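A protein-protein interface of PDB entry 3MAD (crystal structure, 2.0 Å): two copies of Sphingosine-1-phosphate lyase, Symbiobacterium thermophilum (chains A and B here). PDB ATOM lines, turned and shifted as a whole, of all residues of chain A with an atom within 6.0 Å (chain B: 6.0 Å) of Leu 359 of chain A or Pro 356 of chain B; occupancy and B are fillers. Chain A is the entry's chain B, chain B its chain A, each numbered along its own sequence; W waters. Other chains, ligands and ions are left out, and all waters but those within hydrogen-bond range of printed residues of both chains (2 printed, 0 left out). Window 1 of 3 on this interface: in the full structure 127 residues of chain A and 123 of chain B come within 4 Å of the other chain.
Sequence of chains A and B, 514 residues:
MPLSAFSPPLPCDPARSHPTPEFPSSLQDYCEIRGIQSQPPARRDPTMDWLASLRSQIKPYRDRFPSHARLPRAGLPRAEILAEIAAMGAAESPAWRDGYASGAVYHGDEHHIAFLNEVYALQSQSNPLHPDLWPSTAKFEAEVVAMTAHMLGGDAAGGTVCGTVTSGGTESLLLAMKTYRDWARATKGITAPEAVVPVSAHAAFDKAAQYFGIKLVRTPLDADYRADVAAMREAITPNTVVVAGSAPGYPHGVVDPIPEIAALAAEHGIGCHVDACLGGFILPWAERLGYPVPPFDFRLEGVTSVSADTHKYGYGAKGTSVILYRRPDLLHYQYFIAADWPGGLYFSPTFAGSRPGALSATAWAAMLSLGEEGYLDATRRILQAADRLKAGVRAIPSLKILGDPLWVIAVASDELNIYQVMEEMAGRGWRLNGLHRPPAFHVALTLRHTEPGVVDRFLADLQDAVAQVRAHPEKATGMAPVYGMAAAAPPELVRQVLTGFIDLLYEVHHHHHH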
ATOM      1  N   TYR A 120      25.801   3.413  24.809  1.00  0.00           N
ATOM      2  CA  TYR A 120      26.586   2.763  23.764  1.00  0.00           C
ATOM      3  C   TYR A 120      27.810   3.574  23.363  1.00  0.00           C
ATOM      4  O   TYR A 120      28.921   3.050  23.309  1.00  0.00           O
ATOM      5  CB  TYR A 120      25.754   2.479  22.510  1.00  0.00           C
ATOM      6  CG  TYR A 120      26.610   1.838  21.450  1.00  0.00           C
ATOM      7  CD1 TYR A 120      26.772   0.450  21.412  1.00  0.00           C
ATOM      8  CD2 TYR A 120      27.312   2.612  20.528  1.00  0.00           C
ATOM      9  CE1 TYR A 120      27.592  -0.146  20.477  1.00  0.00           C
ATOM     10  CE2 TYR A 120      28.138   2.013  19.579  1.00  0.00           C
ATOM     11  CZ  TYR A 120      28.270   0.630  19.565  1.00  0.00           C
ATOM     12  OH  TYR A 120      29.080   0.017  18.632  1.00  0.00           O
ATOM     13  N   SER A 167      24.219 -13.130  24.504  1.00  0.00           N
ATOM     14  CA  SER A 167      23.886 -12.273  23.377  1.00  0.00           C
ATOM     15  C   SER A 167      22.386 -12.243  23.093  1.00  0.00           C
ATOM     16  O   SER A 167      21.918 -11.462  22.267  1.00  0.00           O
ATOM     17  CB  SER A 167      24.620 -12.744  22.123  1.00  0.00           C
ATOM     18  OG  SER A 167      24.098 -13.997  21.684  1.00  0.00           O
ATOM     19  N   ALA A 317      19.100  -2.609  25.179  1.00  0.00           N
ATOM     20  CA  ALA A 317      19.254  -2.628  23.723  1.00  0.00           C
ATOM     21  C   ALA A 317      19.330  -4.067  23.201  1.00  0.00           C
ATOM     22  O   ALA A 317      19.646  -4.985  23.951  1.00  0.00           O
ATOM     23  CB  ALA A 317      20.496  -1.853  23.307  1.00  0.00           C
ATOM     24  N   LYS A 318      19.041  -4.271  21.919  1.00  0.00           N
ATOM     25  CA  LYS A 318      19.159  -5.613  21.343  1.00  0.00           C
ATOM     26  C   LYS A 318      20.587  -6.119  21.520  1.00  0.00           C
ATOM     27  O   LYS A 318      21.549  -5.354  21.372  1.00  0.00           O
ATOM     28  CB  LYS A 318      18.786  -5.607  19.863  1.00  0.00           C
ATOM     29  CG  LYS A 318      17.283  -5.485  19.585  1.00  0.00           C
ATOM     30  CD  LYS A 318      16.620  -6.861  19.461  1.00  0.00           C
ATOM     31  CE  LYS A 318      16.084  -7.377  20.792  1.00  0.00           C
ATOM     32  NZ  LYS A 318      14.870  -6.630  21.238  1.00  0.00           N
ATOM     33  N   GLY A 319      20.723  -7.399  21.859  1.00  0.00           N
ATOM     34  CA  GLY A 319      22.027  -8.032  21.927  1.00  0.00           C
ATOM     35  C   GLY A 319      22.434  -8.553  23.292  1.00  0.00           C
ATOM     36  O   GLY A 319      23.609  -8.842  23.518  1.00  0.00           O
ATOM     37  N   THR A 320      21.478  -8.672  24.211  1.00  0.00           N
ATOM     38  CA  THR A 320      21.780  -9.221  25.533  1.00  0.00           C
ATOM     39  C   THR A 320      20.648 -10.052  26.126  1.00  0.00           C
ATOM     40  O   THR A 320      19.474  -9.843  25.832  1.00  0.00           O
ATOM     41  CB  THR A 320      22.116  -8.129  26.567  1.00  0.00           C
ATOM     42  OG1 THR A 320      20.911  -7.474  26.971  1.00  0.00           O
ATOM     43  CG2 THR A 320      23.100  -7.118  26.013  1.00  0.00           C
ATOM     44  N   PRO A 356      30.505  -7.314  22.020  1.00  0.00           N
ATOM     45  CA  PRO A 356      30.230  -5.870  22.108  1.00  0.00           C
ATOM     46  C   PRO A 356      29.862  -5.474  23.535  1.00  0.00           C
ATOM     47  O   PRO A 356      28.677  -5.486  23.880  1.00  0.00           O
ATOM     48  CB  PRO A 356      29.004  -5.676  21.208  1.00  0.00           C
ATOM     49  CG  PRO A 356      28.513  -7.069  20.840  1.00  0.00           C
ATOM     50  CD  PRO A 356      29.332  -8.083  21.570  1.00  0.00           C
ATOM     51  N   GLY A 357      30.857  -5.132  24.346  1.00  0.00           N
ATOM     52  CA  GLY A 357      30.619  -4.777  25.737  1.00  0.00           C
ATOM     53  C   GLY A 357      29.590  -3.681  25.921  1.00  0.00           C
ATOM     54  O   GLY A 357      28.854  -3.659  26.916  1.00  0.00           O
ATOM     55  N   ALA A 358      29.528  -2.763  24.962  1.00  0.00           N
ATOM     56  CA  ALA A 358      28.599  -1.642  25.056  1.00  0.00           C
ATOM     57  C   ALA A 358      27.160  -2.113  25.269  1.00  0.00           C
ATOM     58  O   ALA A 358      26.366  -1.417  25.904  1.00  0.00           O
ATOM     59  CB  ALA A 358      28.693  -0.767  23.823  1.00  0.00           C
ATOM     60  N   LEU A 359      26.821  -3.296  24.752  1.00  0.00           N
ATOM     61  CA  LEU A 359      25.450  -3.789  24.885  1.00  0.00           C
ATOM     62  C   LEU A 359      25.135  -4.234  26.307  1.00  0.00           C
ATOM     63  O   LEU A 359      24.007  -4.077  26.781  1.00  0.00           O
ATOM     64  CB  LEU A 359      25.148  -4.893  23.872  1.00  0.00           C
ATOM     65  CG  LEU A 359      25.448  -4.513  22.421  1.00  0.00           C
ATOM     66  CD1 LEU A 359      25.076  -5.648  21.475  1.00  0.00           C
ATOM     67  CD2 LEU A 359      24.729  -3.221  22.032  1.00  0.00           C
ATOM     68  N   SER A 360      26.131  -4.790  26.986  1.00  0.00           N
ATOM     69  CA  SER A 360      25.995  -5.091  28.407  1.00  0.00           C
ATOM     70  C   SER A 360      25.788  -3.808  29.202  1.00  0.00           C
ATOM     71  O   SER A 360      25.014  -3.772  30.157  1.00  0.00           O
ATOM     72  CB  SER A 360      27.236  -5.825  28.913  1.00  0.00           C
ATOM     73  OG  SER A 360      27.396  -7.050  28.220  1.00  0.00           O
ATOM     74  N   ALA A 361      26.481  -2.750  28.800  1.00  0.00           N
ATOM     75  CA  ALA A 361      26.298  -1.443  29.433  1.00  0.00           C
ATOM     76  C   ALA A 361      24.843  -0.974  29.330  1.00  0.00           C
ATOM     77  O   ALA A 361      24.281  -0.471  30.302  1.00  0.00           O
ATOM     78  CB  ALA A 361      27.230  -0.416  28.816  1.00  0.00           C
ATOM     79  N   THR A 362      24.232  -1.144  28.158  1.00  0.00           N
ATOM     80  CA  THR A 362      22.849  -0.695  27.963  1.00  0.00           C
ATOM     81  C   THR A 362      21.852  -1.485  28.819  1.00  0.00           C
ATOM     82  O   THR A 362      20.856  -0.926  29.281  1.00  0.00           O
ATOM     83  CB  THR A 362      22.410  -0.728  26.473  1.00  0.00           C
ATOM     84  OG1 THR A 362      22.204  -2.081  26.045  1.00  0.00           O
ATOM     85  CG2 THR A 362      23.461  -0.063  25.585  1.00  0.00           C
ATOM     86  N   ALA A 363      22.112  -2.777  29.023  1.00  0.00           N
ATOM     87  CA  ALA A 363      21.240  -3.596  29.867  1.00  0.00           C
ATOM     88  C   ALA A 363      21.303  -3.133  31.328  1.00  0.00           C
ATOM     89  O   ALA A 363      20.278  -2.944  31.985  1.00  0.00           O
ATOM     90  CB  ALA A 363      21.612  -5.060  29.751  1.00  0.00           C
ATOM     91  N   TRP A 364      22.519  -2.961  31.828  1.00  0.00           N
ATOM     92  CA  TRP A 364      22.762  -2.411  33.158  1.00  0.00           C
ATOM     93  C   TRP A 364      22.106  -1.031  33.314  1.00  0.00           C
ATOM     94  O   TRP A 364      21.376  -0.774  34.281  1.00  0.00           O
ATOM     95  CB  TRP A 364      24.272  -2.305  33.355  1.00  0.00           C
ATOM     96  CG  TRP A 364      24.751  -1.826  34.694  1.00  0.00           C
ATOM     97  CD1 TRP A 364      24.907  -2.571  35.827  1.00  0.00           C
ATOM     98  CD2 TRP A 364      25.194  -0.499  35.022  1.00  0.00           C
ATOM     99  NE1 TRP A 364      25.410  -1.784  36.845  1.00  0.00           N
ATOM    100  CE2 TRP A 364      25.589  -0.510  36.373  1.00  0.00           C
ATOM    101  CE3 TRP A 364      25.283   0.698  34.304  1.00  0.00           C
ATOM    102  CZ2 TRP A 364      26.069   0.628  37.019  1.00  0.00           C
ATOM    103  CZ3 TRP A 364      25.766   1.824  34.948  1.00  0.00           C
ATOM    104  CH2 TRP A 364      26.146   1.782  36.292  1.00  0.00           C
ATOM    105  N   TYR B 120      25.289   3.638  14.887  1.00  0.00           N
ATOM    106  CA  TYR B 120      24.607   2.845  15.900  1.00  0.00           C
ATOM    107  C   TYR B 120      23.300   3.502  16.344  1.00  0.00           C
ATOM    108  O   TYR B 120      22.253   2.858  16.367  1.00  0.00           O
ATOM    109  CB  TYR B 120      25.487   2.601  17.132  1.00  0.00           C
ATOM    110  CG  TYR B 120      24.708   1.838  18.166  1.00  0.00           C
ATOM    111  CD1 TYR B 120      24.674   0.446  18.144  1.00  0.00           C
ATOM    112  CD2 TYR B 120      23.936   2.502  19.112  1.00  0.00           C
ATOM    113  CE1 TYR B 120      23.928  -0.260  19.059  1.00  0.00           C
ATOM    114  CE2 TYR B 120      23.190   1.803  20.038  1.00  0.00           C
ATOM    115  CZ  TYR B 120      23.190   0.419  20.003  1.00  0.00           C
ATOM    116  OH  TYR B 120      22.445  -0.290  20.909  1.00  0.00           O
ATOM    117  N   SER B 126      17.277  -1.786  15.320  1.00  0.00           N
ATOM    118  CA  SER B 126      17.292  -2.812  14.289  1.00  0.00           C
ATOM    119  C   SER B 126      17.472  -4.212  14.855  1.00  0.00           C
ATOM    120  O   SER B 126      18.372  -4.456  15.658  1.00  0.00           O
ATOM    121  CB  SER B 126      18.400  -2.539  13.270  1.00  0.00           C
ATOM    122  OG  SER B 126      18.597  -3.688  12.458  1.00  0.00           O
ATOM    123  N   ASN B 127      16.611  -5.124  14.414  1.00  0.00           N
ATOM    124  CA  ASN B 127      16.736  -6.544  14.723  1.00  0.00           C
ATOM    125  C   ASN B 127      16.492  -7.375  13.459  1.00  0.00           C
ATOM    126  O   ASN B 127      15.345  -7.636  13.099  1.00  0.00           O
ATOM    127  CB  ASN B 127      15.738  -6.938  15.817  1.00  0.00           C
ATOM    128  CG  ASN B 127      15.838  -8.400  16.194  1.00  0.00           C
ATOM    129  OD1 ASN B 127      16.645  -9.138  15.631  1.00  0.00           O
ATOM    130  ND2 ASN B 127      15.016  -8.831  17.149  1.00  0.00           N
ATOM    131  N   PRO B 128      17.575  -7.789  12.780  1.00  0.00           N
ATOM    132  CA  PRO B 128      17.526  -8.494  11.489  1.00  0.00           C
ATOM    133  C   PRO B 128      16.775  -9.832  11.539  1.00  0.00           C
ATOM    134  O   PRO B 128      16.683 -10.526  10.523  1.00  0.00           O
ATOM    135  CB  PRO B 128      19.007  -8.729  11.152  1.00  0.00           C
ATOM    136  CG  PRO B 128      19.768  -7.747  12.007  1.00  0.00           C
ATOM    137  CD  PRO B 128      18.956  -7.599  13.258  1.00  0.00           C
ATOM    138  N   THR B 137      18.825  -3.060   7.267  1.00  0.00           N
ATOM    139  CA  THR B 137      19.870  -3.874   7.872  1.00  0.00           C
ATOM    140  C   THR B 137      20.169  -5.132   7.044  1.00  0.00           C
ATOM    141  O   THR B 137      21.309  -5.590   6.982  1.00  0.00           O
ATOM    142  CB  THR B 137      19.507  -4.226   9.327  1.00  0.00           C
ATOM    143  OG1 THR B 137      18.967  -3.059   9.972  1.00  0.00           O
ATOM    144  CG2 THR B 137      20.741  -4.695  10.085  1.00  0.00           C
ATOM    145  N   SER B 354      17.243 -13.151  17.787  1.00  0.00           N
ATOM    146  CA  SER B 354      17.363 -11.693  17.831  1.00  0.00           C
ATOM    147  C   SER B 354      18.838 -11.319  17.817  1.00  0.00           C
ATOM    148  O   SER B 354      19.664 -11.994  18.437  1.00  0.00           O
ATOM    149  CB  SER B 354      16.705 -11.133  19.090  1.00  0.00           C
ATOM    150  OG  SER B 354      15.297 -11.295  19.051  1.00  0.00           O
ATOM    151  N   ARG B 355      19.173 -10.256  17.100  1.00  0.00           N
ATOM    152  CA  ARG B 355      20.549  -9.771  17.074  1.00  0.00           C
ATOM    153  C   ARG B 355      20.584  -8.260  16.858  1.00  0.00           C
ATOM    154  O   ARG B 355      19.615  -7.685  16.363  1.00  0.00           O
ATOM    155  CB  ARG B 355      21.365 -10.523  16.015  1.00  0.00           C
ATOM    156  CG  ARG B 355      20.653 -10.727  14.707  1.00  0.00           C
ATOM    157  CD  ARG B 355      21.177 -11.978  13.982  1.00  0.00           C
ATOM    158  NE  ARG B 355      20.745 -12.007  12.584  1.00  0.00           N
ATOM    159  CZ  ARG B 355      19.666 -12.650  12.136  1.00  0.00           C
ATOM    160  NH1 ARG B 355      18.892 -13.342  12.970  1.00  0.00           N
ATOM    161  NH2 ARG B 355      19.362 -12.612  10.844  1.00  0.00           N
ATOM    162  N   PRO B 356      21.696  -7.610  17.242  1.00  0.00           N
ATOM    163  CA  PRO B 356      21.803  -6.144  17.159  1.00  0.00           C
ATOM    164  C   PRO B 356      22.170  -5.693  15.749  1.00  0.00           C
ATOM    165  O   PRO B 356      23.360  -5.580  15.437  1.00  0.00           O
ATOM    166  CB  PRO B 356      22.958  -5.812  18.111  1.00  0.00           C
ATOM    167  CG  PRO B 356      23.569  -7.148  18.531  1.00  0.00           C
ATOM    168  CD  PRO B 356      22.952  -8.226  17.701  1.00  0.00           C
ATOM    169  N   GLY B 357      21.166  -5.453  14.911  1.00  0.00           N
ATOM    170  CA  GLY B 357      21.393  -5.046  13.534  1.00  0.00           C
ATOM    171  C   GLY B 357      22.213  -3.772  13.402  1.00  0.00           C
ATOM    172  O   GLY B 357      22.863  -3.536  12.378  1.00  0.00           O
ATOM    173  N   ALA B 358      22.176  -2.937  14.434  1.00  0.00           N
ATOM    174  CA  ALA B 358      22.976  -1.716  14.433  1.00  0.00           C
ATOM    175  C   ALA B 358      24.463  -2.009  14.217  1.00  0.00           C
ATOM    176  O   ALA B 358      25.168  -1.218  13.593  1.00  0.00           O
ATOM    177  CB  ALA B 358      22.779  -0.958  15.715  1.00  0.00           C
ATOM    178  N   LEU B 359      24.945  -3.139  14.736  1.00  0.00           N
ATOM    179  CA  LEU B 359      26.366  -3.457  14.611  1.00  0.00           C
ATOM    180  C   LEU B 359      26.740  -3.851  13.182  1.00  0.00           C
ATOM    181  O   LEU B 359      27.836  -3.547  12.704  1.00  0.00           O
ATOM    182  CB  LEU B 359      26.785  -4.541  15.606  1.00  0.00           C
ATOM    183  CG  LEU B 359      26.577  -4.219  17.089  1.00  0.00           C
ATOM    184  CD1 LEU B 359      27.103  -5.355  17.950  1.00  0.00           C
ATOM    185  CD2 LEU B 359      27.228  -2.879  17.488  1.00  0.00           C
ATOM    186  N   SER B 360      25.824  -4.530  12.499  1.00  0.00           N
ATOM    187  CA  SER B 360      25.984  -4.789  11.073  1.00  0.00           C
ATOM    188  C   SER B 360      26.054  -3.479  10.284  1.00  0.00           C
ATOM    189  O   SER B 360      26.844  -3.346   9.353  1.00  0.00           O
ATOM    190  CB  SER B 360      24.820  -5.641  10.565  1.00  0.00           C
ATOM    191  OG  SER B 360      24.835  -6.915  11.189  1.00  0.00           O
ATOM    192  N   ALA B 361      25.225  -2.512  10.660  1.00  0.00           N
ATOM    193  CA  ALA B 361      25.272  -1.194  10.026  1.00  0.00           C
ATOM    194  C   ALA B 361      26.664  -0.573  10.152  1.00  0.00           C
ATOM    195  O   ALA B 361      27.165   0.022   9.201  1.00  0.00           O
ATOM    196  CB  ALA B 361      24.225  -0.263  10.621  1.00  0.00           C
HETATM  197  O   HOH W   1      21.554  -2.901  19.650  1.00  0.00           O
HETATM  198  O   HOH W   2      22.112 -11.551  19.669  1.00  0.00           O
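The backbone carbonyl oxygen (O) of Leu 359 of chain A sits at hydrogen-bond distance from the side-chain hydroxyl (OG1) of Thr 362 of chain A (2.8 Å).
The backbone NH of Ala 317 of chain A lies close to the side-chain hydroxyl of Thr 362 of chain A (3.3 Å).
The side-chain amide nitrogen (ND2) of Asn 127 of chain B lies within hydrogen-bond range of the side-chain hydroxyl (OG) of Ser 354 of chain B, at 3.1 Å.
The side-chain amide oxygen (OD1) of Asn 127 of chain B is in hydrogen-bond range of the backbone NH (N) of Arg 355 of chain B, 3.1 Å away.
Among the printed residues, merely in contact across the chains: Tyr 120 of chain A with Tyr 120 of chain B (3.6 Å), Tyr 120 of chain A with Leu 359 of chain B (3.6 Å), Ala 317 of chain A with Tyr 120 of chain B (3.5 Å), Lys 318 of chain A with Asn 127 of chain B (3.4 Å), Lys 318 of chain A with Pro 356 of chain B (3.6 Å), Gly 319 of chain A with Pro 356 of chain B (3.8 Å), Pro 356 of chain A with Leu 359 of chain B (3.6 Å), Leu 359 of chain A with Tyr 120 of chain B (3.9 Å) and Leu 359 of chain A with Pro 356 of chain B (3.6 Å).
Leu 359 of chain A touches just these residues of chain B: Tyr 120 and Pro 356.
Of chain A, only Lys 318 (3.6 Å), Gly 319 (3.8 Å) and Leu 359 (3.6 Å) come within 4 Å of Pro 356 of chain B.
Printed residues of chain B within 4 Å of Tyr 120 of chain A: Tyr 120 and Leu 359.
Of the printed residues of chain B, Pro 356 of chain A touches Leu 359.
Of the printed residues of chain A, Leu 359 of chain B touches Tyr 120 and Pro 356.
Printed residues of chain B within 4 Å of Gly 319 of chain A: Pro 356 (3.8 Å).
Printed residues of chain A within 4 Å of Asn 127 of chain B: Lys 318 (3.4 Å).
Thr 320 of chain A touches none of the printed residues of chain B.
Thr 362 of chain A touches none of the printed residues of chain B.
The nearest residue of chain B that does not touch Leu 359 of chain A is Leu 359 of chain B (4.1 Å).
The nearest residue of chain A that does not touch Pro 356 of chain B is Pro 356 of chain A (5.5 Å).
The nearest printed residue of chain B that does not touch Lys 318 of chain A is Arg 355 of chain B (4.2 Å).
Printed residues of chain B that touch a printed residue of chain A: Tyr 120, Asn 127, Pro 356 and Leu 359.
Of the 15 printed residues of chain A, 6 touch a printed residue of chain B.
Printed residues of chain A that touch a printed residue of chain B: Tyr 120, Ala 317, Lys 318, Gly 319, Pro 356 and Leu 359.
Hydrophobic or aromatic side chains of chain A that line the printed part of chain B: Tyr 120, Ala 317, Pro 356 and Leu 359.
Tyr 120 of chain B touches its own counterpart, Tyr 120 of chain A.
Tyr 120 of chain A touches Leu 359 of chain B, and with the chains exchanged Leu 359 of chain A touches Tyr 120 of chain B.
Pro 356 of chain A touches Leu 359 of chain B, and with the chains exchanged Leu 359 of chain A touches Pro 356 of chain B.
Positions printed for both chains: 120, 356, 357, 358, 359, 360 and 361.
Water W2 lies within hydrogen-bond range of the backbone carbonyl oxygen of Ser 167 of chain A and the backbone carbonyl oxygen of Ser 354 of chain B.
Water W1 lies within hydrogen-bond range of the backbone carbonyl oxygen (O) of Lys 318 of chain A (3.0 Å) and the side-chain hydroxyl (OH) of Tyr 120 of chain B (3.0 Å).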
